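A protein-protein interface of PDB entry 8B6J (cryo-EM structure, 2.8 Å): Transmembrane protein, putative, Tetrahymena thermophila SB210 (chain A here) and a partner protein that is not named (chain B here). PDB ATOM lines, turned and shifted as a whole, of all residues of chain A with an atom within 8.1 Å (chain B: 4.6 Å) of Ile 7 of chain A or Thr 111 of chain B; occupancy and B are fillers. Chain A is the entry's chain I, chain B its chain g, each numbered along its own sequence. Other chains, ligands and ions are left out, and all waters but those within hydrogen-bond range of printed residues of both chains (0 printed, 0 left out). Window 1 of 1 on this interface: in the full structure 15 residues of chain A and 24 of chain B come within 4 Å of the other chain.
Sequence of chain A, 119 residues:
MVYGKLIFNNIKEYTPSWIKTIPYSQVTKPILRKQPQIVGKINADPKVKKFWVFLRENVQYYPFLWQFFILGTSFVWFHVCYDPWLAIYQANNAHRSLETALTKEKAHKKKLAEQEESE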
ATOM      1  N   VAL A   2     -21.697 -13.928  12.639  1.00  0.00           N
ATOM      2  CA  VAL A   2     -21.446 -13.019  11.532  1.00  0.00           C
ATOM      3  C   VAL A   2     -22.431 -11.858  11.574  1.00  0.00           C
ATOM      4  O   VAL A   2     -22.342 -10.928  10.776  1.00  0.00           O
ATOM      5  CB  VAL A   2     -21.533 -13.752  10.181  1.00  0.00           C
ATOM      6  CG1 VAL A   2     -20.834 -15.096  10.258  1.00  0.00           C
ATOM      7  CG2 VAL A   2     -22.982 -13.923   9.754  1.00  0.00           C
ATOM      8  N   TYR A   3     -23.377 -11.918  12.512  1.00  0.00           N
ATOM      9  CA  TYR A   3     -24.433 -10.914  12.565  1.00  0.00           C
ATOM     10  C   TYR A   3     -23.896  -9.568  13.035  1.00  0.00           C
ATOM     11  O   TYR A   3     -24.198  -8.527  12.439  1.00  0.00           O
ATOM     12  CB  TYR A   3     -25.559 -11.396  13.479  1.00  0.00           C
ATOM     13  CG  TYR A   3     -26.937 -11.220  12.890  1.00  0.00           C
ATOM     14  CD1 TYR A   3     -27.483 -12.183  12.056  1.00  0.00           C
ATOM     15  CD2 TYR A   3     -27.694 -10.091  13.170  1.00  0.00           C
ATOM     16  CE1 TYR A   3     -28.742 -12.029  11.516  1.00  0.00           C
ATOM     17  CE2 TYR A   3     -28.955  -9.927  12.635  1.00  0.00           C
ATOM     18  CZ  TYR A   3     -29.474 -10.899  11.808  1.00  0.00           C
ATOM     19  OH  TYR A   3     -30.730 -10.741  11.271  1.00  0.00           O
ATOM     20  N   GLY A   4     -23.098  -9.565  14.097  1.00  0.00           N
ATOM     21  CA  GLY A   4     -22.609  -8.307  14.640  1.00  0.00           C
ATOM     22  C   GLY A   4     -21.850  -8.513  15.932  1.00  0.00           C
ATOM     23  O   GLY A   4     -21.265  -9.576  16.166  1.00  0.00           O
ATOM     24  N   LYS A   5     -21.864  -7.476  16.766  1.00  0.00           N
ATOM     25  CA  LYS A   5     -21.130  -7.502  18.020  1.00  0.00           C
ATOM     26  C   LYS A   5     -21.792  -8.452  19.016  1.00  0.00           C
ATOM     27  O   LYS A   5     -22.938  -8.880  18.852  1.00  0.00           O
ATOM     28  CB  LYS A   5     -21.050  -6.102  18.626  1.00  0.00           C
ATOM     29  CG  LYS A   5     -20.170  -5.135  17.862  1.00  0.00           C
ATOM     30  CD  LYS A   5     -20.061  -3.813  18.599  1.00  0.00           C
ATOM     31  CE  LYS A   5     -19.105  -2.864  17.903  1.00  0.00           C
ATOM     32  NZ  LYS A   5     -18.944  -1.596  18.662  1.00  0.00           N
ATOM     33  N   LEU A   6     -21.042  -8.784  20.063  1.00  0.00           N
ATOM     34  CA  LEU A   6     -21.595  -9.542  21.175  1.00  0.00           C
ATOM     35  C   LEU A   6     -22.480  -8.639  22.022  1.00  0.00           C
ATOM     36  O   LEU A   6     -22.079  -7.534  22.396  1.00  0.00           O
ATOM     37  CB  LEU A   6     -20.477 -10.132  22.031  1.00  0.00           C
ATOM     38  CG  LEU A   6     -19.824 -11.420  21.528  1.00  0.00           C
ATOM     39  CD1 LEU A   6     -19.246 -11.235  20.141  1.00  0.00           C
ATOM     40  CD2 LEU A   6     -18.747 -11.868  22.496  1.00  0.00           C
ATOM     41  N   ILE A   7     -23.684  -9.113  22.327  1.00  0.00           N
ATOM     42  CA  ILE A   7     -24.650  -8.374  23.128  1.00  0.00           C
ATOM     43  C   ILE A   7     -24.906  -9.163  24.403  1.00  0.00           C
ATOM     44  O   ILE A   7     -25.247 -10.350  24.346  1.00  0.00           O
ATOM     45  CB  ILE A   7     -25.957  -8.117  22.356  1.00  0.00           C
ATOM     46  CG1 ILE A   7     -26.392  -9.371  21.593  1.00  0.00           C
ATOM     47  CG2 ILE A   7     -25.776  -6.940  21.407  1.00  0.00           C
ATOM     48  CD1 ILE A   7     -27.719  -9.233  20.881  1.00  0.00           C
ATOM     49  N   PHE A   8     -24.730  -8.506  25.544  1.00  0.00           N
ATOM     50  CA  PHE A   8     -24.808  -9.162  26.840  1.00  0.00           C
ATOM     51  C   PHE A   8     -26.236  -9.080  27.381  1.00  0.00           C
ATOM     52  O   PHE A   8     -27.168  -8.679  26.682  1.00  0.00           O
ATOM     53  CB  PHE A   8     -23.788  -8.544  27.793  1.00  0.00           C
ATOM     54  CG  PHE A   8     -22.364  -8.773  27.380  1.00  0.00           C
ATOM     55  CD1 PHE A   8     -21.730  -9.967  27.669  1.00  0.00           C
ATOM     56  CD2 PHE A   8     -21.660  -7.797  26.700  1.00  0.00           C
ATOM     57  CE1 PHE A   8     -20.425 -10.183  27.290  1.00  0.00           C
ATOM     58  CE2 PHE A   8     -20.353  -8.008  26.319  1.00  0.00           C
ATOM     59  CZ  PHE A   8     -19.735  -9.203  26.614  1.00  0.00           C
ATOM     60  N   ASN A   9     -26.414  -9.464  28.644  1.00  0.00           N
ATOM     61  CA  ASN A   9     -27.738  -9.605  29.237  1.00  0.00           C
ATOM     62  C   ASN A   9     -28.351  -8.281  29.669  1.00  0.00           C
ATOM     63  O   ASN A   9     -29.427  -8.291  30.275  1.00  0.00           O
ATOM     64  CB  ASN A   9     -27.671 -10.550  30.440  1.00  0.00           C
ATOM     65  CG  ASN A   9     -26.726 -10.055  31.516  1.00  0.00           C
ATOM     66  OD1 ASN A   9     -25.513 -10.237  31.423  1.00  0.00           O
ATOM     67  ND2 ASN A   9     -27.277  -9.428  32.548  1.00  0.00           N
ATOM     68  N   ASN A  10     -27.705  -7.149  29.391  1.00  0.00           N
ATOM     69  CA  ASN A  10     -28.301  -5.860  29.715  1.00  0.00           C
ATOM     70  C   ASN A  10     -29.385  -5.450  28.728  1.00  0.00           C
ATOM     71  O   ASN A  10     -30.079  -4.458  28.975  1.00  0.00           O
ATOM     72  CB  ASN A  10     -27.225  -4.774  29.777  1.00  0.00           C
ATOM     73  CG  ASN A  10     -26.485  -4.609  28.470  1.00  0.00           C
ATOM     74  OD1 ASN A  10     -26.222  -5.582  27.767  1.00  0.00           O
ATOM     75  ND2 ASN A  10     -26.142  -3.372  28.138  1.00  0.00           N
ATOM     76  N   ILE A  11     -29.546  -6.178  27.626  1.00  0.00           N
ATOM     77  CA  ILE A  11     -30.621  -5.932  26.674  1.00  0.00           C
ATOM     78  C   ILE A  11     -31.821  -6.758  27.125  1.00  0.00           C
ATOM     79  O   ILE A  11     -31.796  -7.989  27.067  1.00  0.00           O
ATOM     80  CB  ILE A  11     -30.202  -6.293  25.244  1.00  0.00           C
ATOM     81  CG1 ILE A  11     -28.861  -5.641  24.894  1.00  0.00           C
ATOM     82  CG2 ILE A  11     -31.275  -5.867  24.254  1.00  0.00           C
ATOM     83  CD1 ILE A  11     -28.852  -4.130  24.999  1.00  0.00           C
ATOM     84  N   GLU A  13     -35.133  -6.884  26.032  1.00  0.00           N
ATOM     85  CA  GLU A  13     -35.998  -7.500  25.039  1.00  0.00           C
ATOM     86  C   GLU A  13     -35.322  -8.718  24.422  1.00  0.00           C
ATOM     87  O   GLU A  13     -34.111  -8.724  24.184  1.00  0.00           O
ATOM     88  CB  GLU A  13     -36.359  -6.492  23.950  1.00  0.00           C
ATOM     89  CG  GLU A  13     -37.052  -5.241  24.466  1.00  0.00           C
ATOM     90  CD  GLU A  13     -38.408  -5.530  25.077  1.00  0.00           C
ATOM     91  OE1 GLU A  13     -38.855  -6.694  25.020  1.00  0.00           O
ATOM     92  OE2 GLU A  13     -39.031  -4.591  25.614  1.00  0.00           O
ATOM     93  N   TYR A  14     -36.115  -9.762  24.167  1.00  0.00           N
ATOM     94  CA  TYR A  14     -35.564 -10.963  23.552  1.00  0.00           C
ATOM     95  C   TYR A  14     -35.029 -10.669  22.158  1.00  0.00           C
ATOM     96  O   TYR A  14     -33.977 -11.187  21.767  1.00  0.00           O
ATOM     97  CB  TYR A  14     -36.620 -12.065  23.493  1.00  0.00           C
ATOM     98  CG  TYR A  14     -36.115 -13.331  22.842  1.00  0.00           C
ATOM     99  CD1 TYR A  14     -35.377 -14.257  23.563  1.00  0.00           C
ATOM    100  CD2 TYR A  14     -36.365 -13.595  21.503  1.00  0.00           C
ATOM    101  CE1 TYR A  14     -34.907 -15.411  22.971  1.00  0.00           C
ATOM    102  CE2 TYR A  14     -35.901 -14.747  20.903  1.00  0.00           C
ATOM    103  CZ  TYR A  14     -35.173 -15.651  21.642  1.00  0.00           C
ATOM    104  OH  TYR A  14     -34.708 -16.800  21.048  1.00  0.00           O
ATOM    105  N   THR A  15     -35.743  -9.855  21.389  1.00  0.00           N
ATOM    106  CA  THR A  15     -35.275  -9.426  20.077  1.00  0.00           C
ATOM    107  C   THR A  15     -34.838  -7.971  20.160  1.00  0.00           C
ATOM    108  O   THR A  15     -35.692  -7.084  20.314  1.00  0.00           O
ATOM    109  CB  THR A  15     -36.373  -9.593  19.026  1.00  0.00           C
ATOM    110  OG1 THR A  15     -36.709 -10.979  18.901  1.00  0.00           O
ATOM    111  CG2 THR A  15     -35.907  -9.067  17.678  1.00  0.00           C
ATOM    112  N   PRO A  16     -33.543  -7.667  20.074  1.00  0.00           N
ATOM    113  CA  PRO A  16     -33.118  -6.266  20.126  1.00  0.00           C
ATOM    114  C   PRO A  16     -33.723  -5.459  18.987  1.00  0.00           C
ATOM    115  O   PRO A  16     -34.004  -5.979  17.906  1.00  0.00           O
ATOM    116  CB  PRO A  16     -31.594  -6.351  20.006  1.00  0.00           C
ATOM    117  CG  PRO A  16     -31.254  -7.711  20.488  1.00  0.00           C
ATOM    118  CD  PRO A  16     -32.394  -8.588  20.080  1.00  0.00           C
ATOM    119  N   TRP A  18     -32.501  -3.169  17.056  1.00  0.00           N
ATOM    120  CA  TRP A  18     -31.692  -2.933  15.866  1.00  0.00           C
ATOM    121  C   TRP A  18     -31.717  -4.091  14.878  1.00  0.00           C
ATOM    122  O   TRP A  18     -31.257  -3.918  13.745  1.00  0.00           O
ATOM    123  CB  TRP A  18     -30.246  -2.637  16.264  1.00  0.00           C
ATOM    124  CG  TRP A  18     -29.571  -3.749  16.996  1.00  0.00           C
ATOM    125  CD1 TRP A  18     -29.015  -4.870  16.454  1.00  0.00           C
ATOM    126  CD2 TRP A  18     -29.366  -3.842  18.409  1.00  0.00           C
ATOM    127  NE1 TRP A  18     -28.480  -5.657  17.442  1.00  0.00           N
ATOM    128  CE2 TRP A  18     -28.683  -5.047  18.652  1.00  0.00           C
ATOM    129  CE3 TRP A  18     -29.695  -3.024  19.491  1.00  0.00           C
ATOM    130  CZ2 TRP A  18     -28.323  -5.453  19.932  1.00  0.00           C
ATOM    131  CZ3 TRP A  18     -29.337  -3.429  20.761  1.00  0.00           C
ATOM    132  CH2 TRP A  18     -28.658  -4.632  20.971  1.00  0.00           C
ATOM    133  N   ILE A  19     -32.229  -5.253  15.264  1.00  0.00           N
ATOM    134  CA  ILE A  19     -32.288  -6.394  14.358  1.00  0.00           C
ATOM    135  C   ILE A  19     -33.415  -6.178  13.357  1.00  0.00           C
ATOM    136  O   ILE A  19     -34.547  -5.856  13.734  1.00  0.00           O
ATOM    137  CB  ILE A  19     -32.470  -7.703  15.140  1.00  0.00           C
ATOM    138  CG1 ILE A  19     -31.144  -8.082  15.807  1.00  0.00           C
ATOM    139  CG2 ILE A  19     -32.976  -8.810  14.217  1.00  0.00           C
ATOM    140  CD1 ILE A  19     -31.189  -9.354  16.605  1.00  0.00           C
ATOM    141  N   PHE B  88     -16.595 -18.939  19.094  1.00  0.00           N
ATOM    142  CA  PHE B  88     -17.032 -19.988  20.007  1.00  0.00           C
ATOM    143  C   PHE B  88     -16.797 -21.316  19.306  1.00  0.00           C
ATOM    144  O   PHE B  88     -17.472 -21.625  18.318  1.00  0.00           O
ATOM    145  CB  PHE B  88     -18.505 -19.830  20.385  1.00  0.00           C
ATOM    146  CG  PHE B  88     -18.833 -18.519  21.036  1.00  0.00           C
ATOM    147  CD1 PHE B  88     -17.944 -17.917  21.906  1.00  0.00           C
ATOM    148  CD2 PHE B  88     -20.036 -17.888  20.774  1.00  0.00           C
ATOM    149  CE1 PHE B  88     -18.248 -16.712  22.500  1.00  0.00           C
ATOM    150  CE2 PHE B  88     -20.343 -16.682  21.367  1.00  0.00           C
ATOM    151  CZ  PHE B  88     -19.448 -16.094  22.231  1.00  0.00           C
ATOM    152  N   LEU B 107     -24.498 -13.532  28.599  1.00  0.00           N
ATOM    153  CA  LEU B 107     -24.763 -13.346  27.180  1.00  0.00           C
ATOM    154  C   LEU B 107     -26.255 -13.314  26.885  1.00  0.00           C
ATOM    155  O   LEU B 107     -27.042 -14.037  27.503  1.00  0.00           O
ATOM    156  CB  LEU B 107     -24.103 -14.452  26.358  1.00  0.00           C
ATOM    157  CG  LEU B 107     -22.793 -14.075  25.666  1.00  0.00           C
ATOM    158  CD1 LEU B 107     -21.786 -13.525  26.658  1.00  0.00           C
ATOM    159  CD2 LEU B 107     -22.222 -15.276  24.938  1.00  0.00           C
ATOM    160  N   HIS B 108     -26.632 -12.461  25.940  1.00  0.00           N
ATOM    161  CA  HIS B 108     -27.982 -12.456  25.409  1.00  0.00           C
ATOM    162  C   HIS B 108     -28.202 -13.708  24.557  1.00  0.00           C
ATOM    163  O   HIS B 108     -27.278 -14.176  23.887  1.00  0.00           O
ATOM    164  CB  HIS B 108     -28.201 -11.196  24.577  1.00  0.00           C
ATOM    165  CG  HIS B 108     -29.597 -11.026  24.073  1.00  0.00           C
ATOM    166  ND1 HIS B 108     -30.043 -11.617  22.913  1.00  0.00           N
ATOM    167  CD2 HIS B 108     -30.641 -10.313  24.557  1.00  0.00           C
ATOM    168  CE1 HIS B 108     -31.306 -11.287  22.709  1.00  0.00           C
ATOM    169  NE2 HIS B 108     -31.693 -10.496  23.692  1.00  0.00           N
ATOM    170  N   PRO B 109     -29.415 -14.273  24.562  1.00  0.00           N
ATOM    171  CA  PRO B 109     -29.607 -15.562  23.872  1.00  0.00           C
ATOM    172  C   PRO B 109     -29.217 -15.544  22.405  1.00  0.00           C
ATOM    173  O   PRO B 109     -28.695 -16.545  21.897  1.00  0.00           O
ATOM    174  CB  PRO B 109     -31.107 -15.829  24.055  1.00  0.00           C
ATOM    175  CG  PRO B 109     -31.474 -15.095  25.278  1.00  0.00           C
ATOM    176  CD  PRO B 109     -30.631 -13.860  25.284  1.00  0.00           C
ATOM    177  N   TYR B 110     -29.454 -14.435  21.701  1.00  0.00           N
ATOM    178  CA  TYR B 110     -29.190 -14.399  20.267  1.00  0.00           C
ATOM    179  C   TYR B 110     -27.720 -14.630  19.948  1.00  0.00           C
ATOM    180  O   TYR B 110     -27.405 -15.250  18.925  1.00  0.00           O
ATOM    181  CB  TYR B 110     -29.650 -13.063  19.679  1.00  0.00           C
ATOM    182  CG  TYR B 110     -31.100 -13.014  19.229  1.00  0.00           C
ATOM    183  CD1 TYR B 110     -31.955 -14.097  19.402  1.00  0.00           C
ATOM    184  CD2 TYR B 110     -31.608 -11.880  18.615  1.00  0.00           C
ATOM    185  CE1 TYR B 110     -33.266 -14.044  18.983  1.00  0.00           C
ATOM    186  CE2 TYR B 110     -32.918 -11.821  18.193  1.00  0.00           C
ATOM    187  CZ  TYR B 110     -33.742 -12.905  18.380  1.00  0.00           C
ATOM    188  OH  TYR B 110     -35.050 -12.847  17.961  1.00  0.00           O
ATOM    189  N   THR B 111     -26.812 -14.173  20.814  1.00  0.00           N
ATOM    190  CA  THR B 111     -25.387 -14.265  20.510  1.00  0.00           C
ATOM    191  C   THR B 111     -24.970 -15.692  20.186  1.00  0.00           C
ATOM    192  O   THR B 111     -24.051 -15.903  19.385  1.00  0.00           O
ATOM    193  CB  THR B 111     -24.560 -13.741  21.683  1.00  0.00           C
ATOM    194  OG1 THR B 111     -24.811 -14.545  22.841  1.00  0.00           O
ATOM    195  CG2 THR B 111     -24.914 -12.302  21.988  1.00  0.00           C
ATOM    196  N   VAL B 112     -25.621 -16.678  20.795  1.00  0.00           N
ATOM    197  CA  VAL B 112     -25.361 -18.077  20.487  1.00  0.00           C
ATOM    198  C   VAL B 112     -26.470 -18.701  19.651  1.00  0.00           C
ATOM    199  O   VAL B 112     -26.205 -19.675  18.927  1.00  0.00           O
ATOM    200  CB  VAL B 112     -25.138 -18.895  21.777  1.00  0.00           C
ATOM    201  CG1 VAL B 112     -26.407 -18.933  22.619  1.00  0.00           C
ATOM    202  CG2 VAL B 112     -24.662 -20.300  21.443  1.00  0.00           C
ATOM    203  N   LEU B 113     -27.694 -18.175  19.714  1.00  0.00           N
ATOM    204  CA  LEU B 113     -28.771 -18.720  18.897  1.00  0.00           C
ATOM    205  C   LEU B 113     -28.472 -18.557  17.415  1.00  0.00           C
ATOM    206  O   LEU B 113     -28.709 -19.475  16.625  1.00  0.00           O
ATOM    207  CB  LEU B 113     -30.093 -18.041  19.251  1.00  0.00           C
ATOM    208  CG  LEU B 113     -31.334 -18.622  18.576  1.00  0.00           C
ATOM    209  CD1 LEU B 113     -31.566 -20.054  19.026  1.00  0.00           C
ATOM    210  CD2 LEU B 113     -32.547 -17.761  18.873  1.00  0.00           C
ATOM    211  N   MET B 115     -25.493 -18.315  16.095  1.00  0.00           N
ATOM    212  CA  MET B 115     -24.400 -19.234  15.802  1.00  0.00           C
ATOM    213  C   MET B 115     -24.928 -20.639  15.547  1.00  0.00           C
ATOM    214  O   MET B 115     -24.480 -21.322  14.619  1.00  0.00           O
ATOM    215  CB  MET B 115     -23.400 -19.245  16.958  1.00  0.00           C
ATOM    216  CG  MET B 115     -22.813 -17.883  17.300  1.00  0.00           C
ATOM    217  SD  MET B 115     -21.521 -17.360  16.159  1.00  0.00           S
ATOM    218  CE  MET B 115     -20.206 -18.485  16.614  1.00  0.00           C
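The backbone NH (N) of His 108 of chain B sits at hydrogen-bond distance from the backbone carbonyl oxygen (O) of Ile 7 of chain A (3.0 Å).
A ring nitrogen (NE2) of His 108 of chain B sits at hydrogen-bond distance from the backbone carbonyl oxygen (O) of Glu 13 of chain A, at 3.0 Å.
A ring nitrogen (NE2) of His 108 of chain B sits close to the backbone carbonyl oxygen (O) of Tyr 14 of chain A (3.1 Å).
OG1 of Thr 15 of chain A lies within hydrogen-bond range of OH of Tyr 110 of chain B (2.7 Å).
ND1 of His 108 of chain B is in hydrogen-bond range of N of Tyr 110 of chain B.
O of His 108 of chain B is in hydrogen-bond range of OG1 of Thr 111 of chain B (2.7 Å).
O of Phe 8 of chain A sits close to OD1 of Asn 10 of chain A (3.4 Å).
Among the printed residues, pairs that only touch across the chains: Ile 7 of chain A with Thr 111 of chain B, Phe 8 of chain A with Leu 107 of chain B, Phe 8 of chain A with His 108 of chain B, Ile 11 of chain A with His 108 of chain B, Tyr 14 of chain A with Pro 109 of chain B, Tyr 14 of chain A with Tyr 110 of chain B, Tyr 14 of chain A with Leu 113 of chain B, Pro 16 of chain A with His 108 of chain B, Pro 16 of chain A with Tyr 110 of chain B and Ile 19 of chain A with Tyr 110 of chain B.
Of chain B, only His 108 (3.0 Å) and Thr 111 (3.1 Å) come within 4 Å of Ile 7 of chain A.
Thr 111 of chain B touches one residue of chain A.
Of the printed residues of chain A, Leu 107 of chain B touches Phe 8 (3.7 Å).
Printed residues of chain B within 4 Å of Glu 13 of chain A: His 108.
Of the printed residues of chain B, Pro 16 of chain A touches His 108 and Tyr 110.
Printed residues of chain B within 4 Å of Tyr 14 of chain A: His 108, Pro 109, Tyr 110 and Leu 113.
Asn 9 of chain A touches none of the printed residues of chain B.
The nearest residue of chain B that does not touch Ile 7 of chain A is Leu 107 of chain B (4.03 Å).
The nearest residue of chain A that does not touch Thr 111 of chain B is Leu 6 of chain A (4.4 Å).
Of the 9 printed residues of chain B, 6 touch a printed residue of chain A.
Hydrophobic or aromatic side chains of chain B that line the printed part of chain A: Leu 107, His 108, Pro 109, Tyr 110 and Leu 113.
Printed residues of chain A that touch a printed residue of chain B: Ile 7, Phe 8, Ile 11, Glu 13, Tyr 14, Thr 15, Pro 16 and Ile 19.
Hydrophobic or aromatic side chains of chain A that line the printed part of chain B: Ile 7, Phe 8, Tyr 14, Pro 16 and Ile 19.
Among the printed residues, 14 pairs touch across the chains.
Among the printed residues, no Asp or Glu carboxylate lies within 4 Å of a Lys or Arg side-chain nitrogen of the other chain.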
